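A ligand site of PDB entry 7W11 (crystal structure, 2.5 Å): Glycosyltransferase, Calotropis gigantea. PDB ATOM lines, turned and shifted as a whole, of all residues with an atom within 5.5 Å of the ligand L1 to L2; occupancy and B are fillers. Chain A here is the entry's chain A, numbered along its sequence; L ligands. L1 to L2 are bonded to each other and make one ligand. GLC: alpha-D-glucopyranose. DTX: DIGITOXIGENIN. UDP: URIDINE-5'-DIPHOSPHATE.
The side-chain amide nitrogen (ND2) of Asn 375 sits at hydrogen-bond distance from an oxygen (O2A) of UDP L3 (2.8 Å).
N of Asn 375 sits at hydrogen-bond distance from O2A of UDP L3.
An oxygen (O5) of GLC L1 sits close to a ring nitrogen (NE2) of His 27.
O4 of GLC L1 sits at hydrogen-bond distance from N of Trp 374.
NE2 of Gln 396 sits at hydrogen-bond distance from O3 of GLC L1 (2.8 Å).
SD of Met 85 lies within hydrogen-bond range of O14 of DTX L2, at 3.5 Å.
O3 of GLC L1 is in hydrogen-bond range of OD1 of Asp 395 (2.8 Å).
An oxygen (O6) of GLC L1 lies within hydrogen-bond range of the side-chain hydroxyl (OG1) of Thr 144 (2.6 Å).
OE2 of Glu 24 lies close to O3B of UDP L3.
O of Thr 144 lies within hydrogen-bond range of O6 of GLC L1.
O of Gly 26 sits at hydrogen-bond distance from O6 of GLC L1, at 3.1 Å.
N of Trp 374 is in hydrogen-bond range of O2A of UDP L3, 3.4 Å away.
A ring nitrogen (NE2) of His 371 sits at hydrogen-bond distance from an oxygen (O3A) of UDP L3 (3.1 Å).
O2 of GLC L1 lies within hydrogen-bond range of O1B of UDP L3.
The side-chain amide nitrogen (ND2) of Asn 375 is in hydrogen-bond range of the backbone carbonyl oxygen (O) of Gly 26.
The backbone NH (N) of Gly 26 lies within hydrogen-bond range of the side-chain carboxylate (OE1) of Glu 24, 3.0 Å away.
A ring nitrogen (ND1) of His 27 sits close to the side-chain hydroxyl of Thr 144, 3.3 Å away.
N of Gly 373 sits close to NE2 of His 371 (3.5 Å).
OD2 of Asp 395 is in hydrogen-bond range of ND2 of Asn 399, 2.8 Å away.
N of His 27 sits close to OE1 of Glu 24 (3.3 Å).
N of Trp 393 is in hydrogen-bond range of OE1 of Gln 396.
The side-chain carboxylate of Glu 24 lies close to an oxygen (O32) of DTX L2, 3.4 Å away.
Phe 22 touches the ligand L1 to L2.
O of Gly 84 touches O21 of DTX L2, 3.6 Å away.
CG of Tyr 88 touches C21 of DTX L2, at 3.4 Å.
NE2 of Gln 145 touches C6 of GLC L1, 3.6 Å away.
CZ of Phe 193 touches C6 of DTX L2 (3.7 Å).
CD2 of Leu 203 touches C19 of DTX L2, 3.5 Å away.
Gly 373 touches the ligand L1 to L2.
ND2 of Asn 375 touches O6 of GLC L1, 3.8 Å away.
CZ3 of Trp 393 touches O2 of GLC L1, 2.8 Å away.
Hydrophobic or aromatic side chains within 4 Å of the ligand L1 to L2: Phe 22, His 27, Met 85, Tyr 88, Phe 193, Leu 203, Trp 374 and Trp 393.
17 residues have an atom within 4 Å of the ligand L1 to L2: Phe 22, Glu 24, Gly 26, His 27, Gly 84, Met 85, Tyr 88, Thr 144, Gln 145, Phe 193, Leu 203, Gly 373, Trp 374, Asn 375, Trp 393, Asp 395 and Gln 396.
Along chain A the residues within 4 Å of the ligand L1 to L2 span positions 22 to 396.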
ATOM      1  N   PHE A  22      -8.014  -4.555  26.248  1.00  0.00           N
ATOM      2  CA  PHE A  22      -8.838  -5.716  26.484  1.00  0.00           C
ATOM      3  C   PHE A  22      -8.304  -6.462  27.711  1.00  0.00           C
ATOM      4  O   PHE A  22      -7.096  -6.588  27.877  1.00  0.00           O
ATOM      5  CB  PHE A  22      -8.867  -6.634  25.269  1.00  0.00           C
ATOM      6  CG  PHE A  22      -9.762  -7.821  25.429  1.00  0.00           C
ATOM      7  CD1 PHE A  22     -11.125  -7.716  25.156  1.00  0.00           C
ATOM      8  CD2 PHE A  22      -9.266  -9.035  25.890  1.00  0.00           C
ATOM      9  CE1 PHE A  22     -11.964  -8.789  25.302  1.00  0.00           C
ATOM     10  CE2 PHE A  22     -10.098 -10.123  26.043  1.00  0.00           C
ATOM     11  CZ  PHE A  22     -11.454 -10.009  25.754  1.00  0.00           C
ATOM     12  N   GLU A  24      -6.859  -9.034  29.248  1.00  0.00           N
ATOM     13  CA  GLU A  24      -6.107 -10.253  29.041  1.00  0.00           C
ATOM     14  C   GLU A  24      -4.634  -9.857  28.952  1.00  0.00           C
ATOM     15  O   GLU A  24      -4.317  -8.844  28.318  1.00  0.00           O
ATOM     16  CB  GLU A  24      -6.562 -10.999  27.774  1.00  0.00           C
ATOM     17  CG  GLU A  24      -5.963 -12.388  27.608  1.00  0.00           C
ATOM     18  CD  GLU A  24      -4.684 -12.428  26.746  1.00  0.00           C
ATOM     19  OE1 GLU A  24      -4.273 -11.391  26.151  1.00  0.00           O
ATOM     20  OE2 GLU A  24      -4.078 -13.528  26.677  1.00  0.00           O
ATOM     21  N   GLY A  26      -1.786 -10.544  27.523  1.00  0.00           N
ATOM     22  CA  GLY A  26      -1.174 -10.144  26.262  1.00  0.00           C
ATOM     23  C   GLY A  26      -1.774  -8.897  25.621  1.00  0.00           C
ATOM     24  O   GLY A  26      -1.245  -8.416  24.610  1.00  0.00           O
ATOM     25  N   HIS A  27      -2.878  -8.375  26.173  1.00  0.00           N
ATOM     26  CA  HIS A  27      -3.342  -7.052  25.794  1.00  0.00           C
ATOM     27  C   HIS A  27      -3.046  -5.996  26.851  1.00  0.00           C
ATOM     28  O   HIS A  27      -2.631  -4.887  26.498  1.00  0.00           O
ATOM     29  CB  HIS A  27      -4.834  -7.089  25.467  1.00  0.00           C
ATOM     30  CG  HIS A  27      -5.139  -7.954  24.292  1.00  0.00           C
ATOM     31  ND1 HIS A  27      -5.574  -7.448  23.097  1.00  0.00           N
ATOM     32  CD2 HIS A  27      -4.979  -9.284  24.117  1.00  0.00           C
ATOM     33  CE1 HIS A  27      -5.711  -8.437  22.233  1.00  0.00           C
ATOM     34  NE2 HIS A  27      -5.352  -9.564  22.830  1.00  0.00           N
ATOM     35  N   GLY A  84     -20.288 -18.637  27.949  1.00  0.00           N
ATOM     36  CA  GLY A  84     -19.641 -18.939  26.690  1.00  0.00           C
ATOM     37  C   GLY A  84     -18.988 -17.716  26.108  1.00  0.00           C
ATOM     38  O   GLY A  84     -19.274 -16.602  26.537  1.00  0.00           O
ATOM     39  N   MET A  85     -18.094 -17.908  25.134  1.00  0.00           N
ATOM     40  CA  MET A  85     -17.324 -16.775  24.623  1.00  0.00           C
ATOM     41  C   MET A  85     -18.240 -15.642  24.194  1.00  0.00           C
ATOM     42  O   MET A  85     -17.933 -14.459  24.401  1.00  0.00           O
ATOM     43  CB  MET A  85     -16.433 -17.210  23.459  1.00  0.00           C
ATOM     44  CG  MET A  85     -15.258 -18.112  23.836  1.00  0.00           C
ATOM     45  SD  MET A  85     -13.830 -18.005  22.703  1.00  0.00           S
ATOM     46  N   TYR A  88     -20.421 -13.748  26.953  1.00  0.00           N
ATOM     47  CA  TYR A  88     -19.456 -12.972  27.716  1.00  0.00           C
ATOM     48  C   TYR A  88     -19.076 -11.710  26.952  1.00  0.00           C
ATOM     49  O   TYR A  88     -18.984 -10.624  27.539  1.00  0.00           O
ATOM     50  CB  TYR A  88     -18.223 -13.845  28.023  1.00  0.00           C
ATOM     51  CG  TYR A  88     -17.010 -13.127  28.613  1.00  0.00           C
ATOM     52  CD1 TYR A  88     -16.794 -13.098  29.993  1.00  0.00           C
ATOM     53  CD2 TYR A  88     -16.038 -12.534  27.786  1.00  0.00           C
ATOM     54  CE1 TYR A  88     -15.673 -12.462  30.528  1.00  0.00           C
ATOM     55  CE2 TYR A  88     -14.913 -11.902  28.308  1.00  0.00           C
ATOM     56  CZ  TYR A  88     -14.736 -11.862  29.679  1.00  0.00           C
ATOM     57  OH  TYR A  88     -13.617 -11.239  30.218  1.00  0.00           O
ATOM     58  N   THR A 144      -2.119  -5.310  19.127  1.00  0.00           N
ATOM     59  CA  THR A 144      -1.197  -6.047  19.982  1.00  0.00           C
ATOM     60  C   THR A 144      -0.646  -7.294  19.286  1.00  0.00           C
ATOM     61  O   THR A 144      -0.291  -8.265  19.953  1.00  0.00           O
ATOM     62  CB  THR A 144      -1.904  -6.428  21.276  1.00  0.00           C
ATOM     63  OG1 THR A 144      -3.076  -7.194  20.951  1.00  0.00           O
ATOM     64  CG2 THR A 144      -2.340  -5.159  22.040  1.00  0.00           C
ATOM     65  N   GLN A 145      -0.592  -7.279  17.963  1.00  0.00           N
ATOM     66  CA  GLN A 145      -0.060  -8.379  17.170  1.00  0.00           C
ATOM     67  C   GLN A 145       0.736  -7.774  16.030  1.00  0.00           C
ATOM     68  O   GLN A 145       0.578  -6.588  15.722  1.00  0.00           O
ATOM     69  CB  GLN A 145      -1.176  -9.280  16.629  1.00  0.00           C
ATOM     70  CG  GLN A 145      -1.735 -10.230  17.632  1.00  0.00           C
ATOM     71  CD  GLN A 145      -2.878 -11.043  17.066  1.00  0.00           C
ATOM     72  OE1 GLN A 145      -2.938 -11.278  15.866  1.00  0.00           O
ATOM     73  NE2 GLN A 145      -3.780 -11.502  17.932  1.00  0.00           N
ATOM     74  N   PHE A 193     -10.973 -23.517  18.091  1.00  0.00           N
ATOM     75  CA  PHE A 193     -12.098 -23.078  18.925  1.00  0.00           C
ATOM     76  C   PHE A 193     -13.438 -23.702  18.502  1.00  0.00           C
ATOM     77  O   PHE A 193     -14.470 -23.423  19.133  1.00  0.00           O
ATOM     78  CB  PHE A 193     -12.137 -21.547  18.918  1.00  0.00           C
ATOM     79  CG  PHE A 193     -10.899 -20.907  19.512  1.00  0.00           C
ATOM     80  CD1 PHE A 193     -10.654 -20.960  20.884  1.00  0.00           C
ATOM     81  CD2 PHE A 193      -9.961 -20.289  18.697  1.00  0.00           C
ATOM     82  CE1 PHE A 193      -9.489 -20.372  21.435  1.00  0.00           C
ATOM     83  CE2 PHE A 193      -8.794 -19.688  19.244  1.00  0.00           C
ATOM     84  CZ  PHE A 193      -8.568 -19.740  20.609  1.00  0.00           C
ATOM     85  N   PHE A 199     -16.663 -16.776  16.191  1.00  0.00           N
ATOM     86  CA  PHE A 199     -16.540 -15.616  17.068  1.00  0.00           C
ATOM     87  C   PHE A 199     -15.101 -15.104  17.099  1.00  0.00           C
ATOM     88  O   PHE A 199     -14.853 -13.911  16.905  1.00  0.00           O
ATOM     89  CB  PHE A 199     -17.002 -15.966  18.486  1.00  0.00           C
ATOM     90  CG  PHE A 199     -16.546 -14.973  19.500  1.00  0.00           C
ATOM     91  CD1 PHE A 199     -17.205 -13.759  19.622  1.00  0.00           C
ATOM     92  CD2 PHE A 199     -15.420 -15.211  20.269  1.00  0.00           C
ATOM     93  CE1 PHE A 199     -16.766 -12.803  20.526  1.00  0.00           C
ATOM     94  CE2 PHE A 199     -14.976 -14.261  21.184  1.00  0.00           C
ATOM     95  CZ  PHE A 199     -15.647 -13.050  21.311  1.00  0.00           C
ATOM     96  N   VAL A 200     -14.144 -16.000  17.370  1.00  0.00           N
ATOM     97  CA  VAL A 200     -12.747 -15.602  17.467  1.00  0.00           C
ATOM     98  C   VAL A 200     -12.289 -14.985  16.142  1.00  0.00           C
ATOM     99  O   VAL A 200     -11.661 -13.923  16.111  1.00  0.00           O
ATOM    100  CB  VAL A 200     -11.857 -16.792  17.868  1.00  0.00           C
ATOM    101  CG1 VAL A 200     -10.426 -16.344  18.030  1.00  0.00           C
ATOM    102  CG2 VAL A 200     -12.352 -17.432  19.143  1.00  0.00           C
ATOM    103  N   LEU A 203     -13.705 -11.620  15.706  1.00  0.00           N
ATOM    104  CA  LEU A 203     -13.104 -10.656  16.605  1.00  0.00           C
ATOM    105  C   LEU A 203     -11.837 -10.050  15.996  1.00  0.00           C
ATOM    106  O   LEU A 203     -11.582  -8.846  16.147  1.00  0.00           O
ATOM    107  CB  LEU A 203     -12.825 -11.334  17.935  1.00  0.00           C
ATOM    108  CG  LEU A 203     -12.031 -10.543  18.975  1.00  0.00           C
ATOM    109  CD1 LEU A 203     -12.884  -9.496  19.674  1.00  0.00           C
ATOM    110  CD2 LEU A 203     -11.426 -11.523  19.985  1.00  0.00           C
ATOM    111  N   LEU A 204     -11.033 -10.870  15.302  1.00  0.00           N
ATOM    112  CA  LEU A 204      -9.737 -10.410  14.795  1.00  0.00           C
ATOM    113  C   LEU A 204      -9.885  -9.674  13.463  1.00  0.00           C
ATOM    114  O   LEU A 204      -9.157  -8.699  13.222  1.00  0.00           O
ATOM    115  CB  LEU A 204      -8.777 -11.599  14.637  1.00  0.00           C
ATOM    116  CG  LEU A 204      -8.043 -12.062  15.899  1.00  0.00           C
ATOM    117  CD1 LEU A 204      -7.470 -10.890  16.707  1.00  0.00           C
ATOM    118  CD2 LEU A 204      -8.942 -12.871  16.748  1.00  0.00           C
ATOM    119  N   ILE A 287      -3.140 -18.092  28.710  1.00  0.00           N
ATOM    120  CA  ILE A 287      -4.419 -18.676  28.332  1.00  0.00           C
ATOM    121  C   ILE A 287      -4.253 -20.141  27.933  1.00  0.00           C
ATOM    122  O   ILE A 287      -4.970 -21.018  28.434  1.00  0.00           O
ATOM    123  CB  ILE A 287      -5.076 -17.883  27.191  1.00  0.00           C
ATOM    124  CG1 ILE A 287      -5.113 -16.376  27.507  1.00  0.00           C
ATOM    125  CG2 ILE A 287      -6.458 -18.439  26.872  1.00  0.00           C
ATOM    126  CD1 ILE A 287      -6.390 -15.899  28.206  1.00  0.00           C
ATOM    127  N   HIS A 371       4.782 -20.746  23.267  1.00  0.00           N
ATOM    128  CA  HIS A 371       3.598 -20.898  22.437  1.00  0.00           C
ATOM    129  C   HIS A 371       3.528 -19.843  21.340  1.00  0.00           C
ATOM    130  O   HIS A 371       2.619 -19.895  20.502  1.00  0.00           O
ATOM    131  CB  HIS A 371       2.360 -20.879  23.328  1.00  0.00           C
ATOM    132  CG  HIS A 371       1.904 -19.516  23.715  1.00  0.00           C
ATOM    133  ND1 HIS A 371       2.696 -18.638  24.417  1.00  0.00           N
ATOM    134  CD2 HIS A 371       0.732 -18.868  23.492  1.00  0.00           C
ATOM    135  CE1 HIS A 371       2.033 -17.510  24.623  1.00  0.00           C
ATOM    136  NE2 HIS A 371       0.841 -17.616  24.065  1.00  0.00           N
ATOM    137  N   CYS A 372       4.460 -18.872  21.332  1.00  0.00           N
ATOM    138  CA  CYS A 372       4.594 -17.853  20.283  1.00  0.00           C
ATOM    139  C   CYS A 372       3.463 -16.822  20.291  1.00  0.00           C
ATOM    140  O   CYS A 372       3.157 -16.264  19.223  1.00  0.00           O
ATOM    141  CB  CYS A 372       4.701 -18.481  18.892  1.00  0.00           C
ATOM    142  SG  CYS A 372       5.953 -19.746  18.676  1.00  0.00           S
ATOM    143  N   GLY A 373       2.816 -16.558  21.423  1.00  0.00           N
ATOM    144  CA  GLY A 373       2.043 -15.327  21.509  1.00  0.00           C
ATOM    145  C   GLY A 373       2.931 -14.167  21.152  1.00  0.00           C
ATOM    146  O   GLY A 373       4.151 -14.235  21.294  1.00  0.00           O
ATOM    147  N   TRP A 374       2.320 -13.070  20.633  1.00  0.00           N
ATOM    148  CA  TRP A 374       3.170 -12.021  20.059  1.00  0.00           C
ATOM    149  C   TRP A 374       3.960 -11.279  21.131  1.00  0.00           C
ATOM    150  O   TRP A 374       5.111 -10.878  20.871  1.00  0.00           O
ATOM    151  CB  TRP A 374       2.363 -11.018  19.234  1.00  0.00           C
ATOM    152  CG  TRP A 374       3.249  -9.914  18.692  1.00  0.00           C
ATOM    153  CD1 TRP A 374       3.173  -8.592  18.990  1.00  0.00           C
ATOM    154  CD2 TRP A 374       4.358 -10.058  17.780  1.00  0.00           C
ATOM    155  NE1 TRP A 374       4.156  -7.890  18.333  1.00  0.00           N
ATOM    156  CE2 TRP A 374       4.900  -8.768  17.585  1.00  0.00           C
ATOM    157  CE3 TRP A 374       4.955 -11.148  17.137  1.00  0.00           C
ATOM    158  CZ2 TRP A 374       6.008  -8.537  16.751  1.00  0.00           C
ATOM    159  CZ3 TRP A 374       6.063 -10.917  16.304  1.00  0.00           C
ATOM    160  CH2 TRP A 374       6.578  -9.616  16.128  1.00  0.00           C
ATOM    161  N   ASN A 375       3.402 -11.103  22.323  1.00  0.00           N
ATOM    162  CA  ASN A 375       4.192 -10.473  23.372  1.00  0.00           C
ATOM    163  C   ASN A 375       5.409 -11.328  23.729  1.00  0.00           C
ATOM    164  O   ASN A 375       6.542 -10.824  23.781  1.00  0.00           O
ATOM    165  CB  ASN A 375       3.330 -10.202  24.603  1.00  0.00           C
ATOM    166  CG  ASN A 375       2.270  -9.179  24.347  1.00  0.00           C
ATOM    167  OD1 ASN A 375       2.529  -7.977  24.365  1.00  0.00           O
ATOM    168  ND2 ASN A 375       1.048  -9.643  24.103  1.00  0.00           N
ATOM    169  N   TRP A 393      -2.718 -21.339  18.864  1.00  0.00           N
ATOM    170  CA  TRP A 393      -3.834 -20.917  18.017  1.00  0.00           C
ATOM    171  C   TRP A 393      -3.747 -19.433  17.675  1.00  0.00           C
ATOM    172  O   TRP A 393      -2.786 -18.738  18.011  1.00  0.00           O
ATOM    173  CB  TRP A 393      -5.177 -21.277  18.678  1.00  0.00           C
ATOM    174  CG  TRP A 393      -5.154 -21.300  20.171  1.00  0.00           C
ATOM    175  CD1 TRP A 393      -5.252 -22.411  20.981  1.00  0.00           C
ATOM    176  CD2 TRP A 393      -4.987 -20.174  21.035  1.00  0.00           C
ATOM    177  NE1 TRP A 393      -5.195 -22.025  22.309  1.00  0.00           N
ATOM    178  CE2 TRP A 393      -5.023 -20.661  22.367  1.00  0.00           C
ATOM    179  CE3 TRP A 393      -4.839 -18.827  20.825  1.00  0.00           C
ATOM    180  CZ2 TRP A 393      -4.897 -19.824  23.470  1.00  0.00           C
ATOM    181  CZ3 TRP A 393      -4.708 -17.994  21.915  1.00  0.00           C
ATOM    182  CH2 TRP A 393      -4.740 -18.494  23.229  1.00  0.00           C
ATOM    183  N   VAL A 394      -4.782 -18.969  16.966  1.00  0.00           N
ATOM    184  CA  VAL A 394      -4.891 -17.621  16.428  1.00  0.00           C
ATOM    185  C   VAL A 394      -3.571 -17.272  15.739  1.00  0.00           C
ATOM    186  O   VAL A 394      -3.157 -17.986  14.817  1.00  0.00           O
ATOM    187  CB  VAL A 394      -5.277 -16.593  17.515  1.00  0.00           C
ATOM    188  CG1 VAL A 394      -5.573 -15.250  16.877  1.00  0.00           C
ATOM    189  CG2 VAL A 394      -6.523 -17.078  18.268  1.00  0.00           C
ATOM    190  N   ASP A 395      -2.908 -16.193  16.186  1.00  0.00           N
ATOM    191  CA  ASP A 395      -1.697 -15.695  15.534  1.00  0.00           C
ATOM    192  C   ASP A 395      -0.422 -16.446  15.898  1.00  0.00           C
ATOM    193  O   ASP A 395       0.608 -16.236  15.250  1.00  0.00           O
ATOM    194  CB  ASP A 395      -1.488 -14.203  15.842  1.00  0.00           C
ATOM    195  CG  ASP A 395      -1.097 -13.971  17.278  1.00  0.00           C
ATOM    196  OD1 ASP A 395      -1.744 -14.595  18.144  1.00  0.00           O
ATOM    197  OD2 ASP A 395      -0.165 -13.198  17.561  1.00  0.00           O
ATOM    198  N   GLN A 396      -0.447 -17.332  16.904  1.00  0.00           N
ATOM    199  CA  GLN A 396       0.766 -18.074  17.236  1.00  0.00           C
ATOM    200  C   GLN A 396       1.316 -18.873  16.059  1.00  0.00           C
ATOM    201  O   GLN A 396       2.540 -19.012  15.936  1.00  0.00           O
ATOM    202  CB  GLN A 396       0.515 -18.993  18.423  1.00  0.00           C
ATOM    203  CG  GLN A 396       0.356 -18.244  19.715  1.00  0.00           C
ATOM    204  CD  GLN A 396      -0.722 -18.854  20.599  1.00  0.00           C
ATOM    205  OE1 GLN A 396      -0.940 -20.068  20.613  1.00  0.00           O
ATOM    206  NE2 GLN A 396      -1.416 -17.993  21.322  1.00  0.00           N
ATOM    207  N   ASN A 399       3.146 -16.395  13.751  1.00  0.00           N
ATOM    208  CA  ASN A 399       4.383 -15.948  14.399  1.00  0.00           C
ATOM    209  C   ASN A 399       5.472 -17.025  14.291  1.00  0.00           C
ATOM    210  O   ASN A 399       6.633 -16.722  13.983  1.00  0.00           O
ATOM    211  CB  ASN A 399       4.097 -15.561  15.857  1.00  0.00           C
ATOM    212  CG  ASN A 399       2.989 -14.497  15.987  1.00  0.00           C
ATOM    213  OD1 ASN A 399       2.745 -13.721  15.057  1.00  0.00           O
ATOM    214  ND2 ASN A 399       2.320 -14.457  17.135  1.00  0.00           N
HETATM  215  C1  GLC L   1      -4.095 -13.249  22.330  1.00  0.00           C
HETATM  216  C2  GLC L   1      -3.356 -14.453  21.862  1.00  0.00           C
HETATM  217  C3  GLC L   1      -1.857 -14.165  21.678  1.00  0.00           C
HETATM  218  C4  GLC L   1      -1.663 -12.835  21.033  1.00  0.00           C
HETATM  219  C5  GLC L   1      -2.188 -11.765  21.980  1.00  0.00           C
HETATM  220  C6  GLC L   1      -2.586 -10.507  21.222  1.00  0.00           C
HETATM  221  O2  GLC L   1      -3.466 -15.582  22.730  1.00  0.00           O
HETATM  222  O3  GLC L   1      -1.291 -15.196  20.863  1.00  0.00           O
HETATM  223  O4  GLC L   1      -0.304 -12.532  20.766  1.00  0.00           O
HETATM  224  O5  GLC L   1      -3.283 -12.198  22.796  1.00  0.00           O
HETATM  225  O6  GLC L   1      -1.959  -9.374  21.779  1.00  0.00           O
HETATM  226  O23 DTX L   2     -15.823 -19.138  27.668  1.00  0.00           O
HETATM  227  C23 DTX L   2     -15.261 -18.073  27.733  1.00  0.00           C
HETATM  228  C22 DTX L   2     -13.848 -17.732  27.651  1.00  0.00           C
HETATM  229  O21 DTX L   2     -15.976 -16.946  27.906  1.00  0.00           O
HETATM  230  C21 DTX L   2     -15.065 -15.826  27.957  1.00  0.00           C
HETATM  231  C20 DTX L   2     -13.724 -16.413  27.655  1.00  0.00           C
HETATM  232  C17 DTX L   2     -12.504 -15.564  27.408  1.00  0.00           C
HETATM  233  C16 DTX L   2     -11.198 -16.160  27.986  1.00  0.00           C
HETATM  234  C13 DTX L   2     -12.209 -15.261  25.912  1.00  0.00           C
HETATM  235  C12 DTX L   2     -11.616 -13.845  25.839  1.00  0.00           C
HETATM  236  C11 DTX L   2     -10.997 -13.552  24.477  1.00  0.00           C
HETATM  237  C18 DTX L   2     -13.426 -15.355  25.004  1.00  0.00           C
HETATM  238  C14 DTX L   2     -11.100 -16.298  25.545  1.00  0.00           C
HETATM  239  C15 DTX L   2     -10.229 -16.331  26.801  1.00  0.00           C
HETATM  240  O14 DTX L   2     -11.730 -17.596  25.415  1.00  0.00           O
HETATM  241  C8  DTX L   2     -10.381 -15.985  24.232  1.00  0.00           C
HETATM  242  C7  DTX L   2      -9.225 -16.965  23.986  1.00  0.00           C
HETATM  243  C9  DTX L   2      -9.869 -14.528  24.126  1.00  0.00           C
HETATM  244  C10 DTX L   2      -9.165 -14.227  22.765  1.00  0.00           C
HETATM  245  C1  DTX L   2      -8.559 -12.804  22.749  1.00  0.00           C
HETATM  246  C19 DTX L   2     -10.149 -14.313  21.593  1.00  0.00           C
HETATM  247  C5  DTX L   2      -8.010 -15.257  22.599  1.00  0.00           C
HETATM  248  C6  DTX L   2      -8.524 -16.691  22.657  1.00  0.00           C
HETATM  249  C4  DTX L   2      -6.851 -15.003  23.581  1.00  0.00           C
HETATM  250  C3  DTX L   2      -6.328 -13.553  23.535  1.00  0.00           C
HETATM  251  C2  DTX L   2      -7.056 -12.792  22.468  1.00  0.00           C
HETATM  252  O32 DTX L   2      -4.893 -13.643  23.426  1.00  0.00           O
HETATM  253  N1  UDP L   3       3.996 -13.613  31.124  1.00  0.00           N
HETATM  254  C2  UDP L   3       4.499 -13.348  32.311  1.00  0.00           C
HETATM  255  N3  UDP L   3       4.867 -14.274  33.161  1.00  0.00           N
HETATM  256  C4  UDP L   3       4.751 -15.538  32.818  1.00  0.00           C
HETATM  257  C5  UDP L   3       4.243 -15.873  31.569  1.00  0.00           C
HETATM  258  C6  UDP L   3       3.853 -14.856  30.710  1.00  0.00           C
HETATM  259  O2  UDP L   3       4.597 -12.011  32.661  1.00  0.00           O
HETATM  260  O4  UDP L   3       5.168 -16.531  33.725  1.00  0.00           O
HETATM  261  C1' UDP L   3       3.627 -12.441  30.296  1.00  0.00           C
HETATM  262  C2' UDP L   3       4.494 -12.380  29.027  1.00  0.00           C
HETATM  263  O2' UDP L   3       5.701 -11.767  29.284  1.00  0.00           O
HETATM  264  C3' UDP L   3       3.567 -11.604  28.046  1.00  0.00           C
HETATM  265  C4' UDP L   3       2.341 -11.948  28.379  1.00  0.00           C
HETATM  266  O4' UDP L   3       2.385 -12.524  29.886  1.00  0.00           O
HETATM  267  O3' UDP L   3       3.718 -10.115  28.187  1.00  0.00           O
HETATM  268  C5' UDP L   3       1.834 -13.075  27.513  1.00  0.00           C
HETATM  269  O5' UDP L   3       1.375 -12.483  26.343  1.00  0.00           O
HETATM  270  PA  UDP L   3       1.444 -13.350  24.953  1.00  0.00           P
HETATM  271  O1A UDP L   3       2.859 -13.841  24.791  1.00  0.00           O
HETATM  272  O2A UDP L   3       1.109 -12.448  23.792  1.00  0.00           O
HETATM  273  O3A UDP L   3       0.456 -14.672  24.958  1.00  0.00           O
HETATM  274  PB  UDP L   3      -1.047 -14.797  25.609  1.00  0.00           P
HETATM  275  O1B UDP L   3      -1.686 -16.018  24.977  1.00  0.00           O
HETATM  276  O2B UDP L   3      -0.905 -14.994  27.092  1.00  0.00           O
HETATM  277  O3B UDP L   3      -1.936 -13.605  25.294  1.00  0.00           O
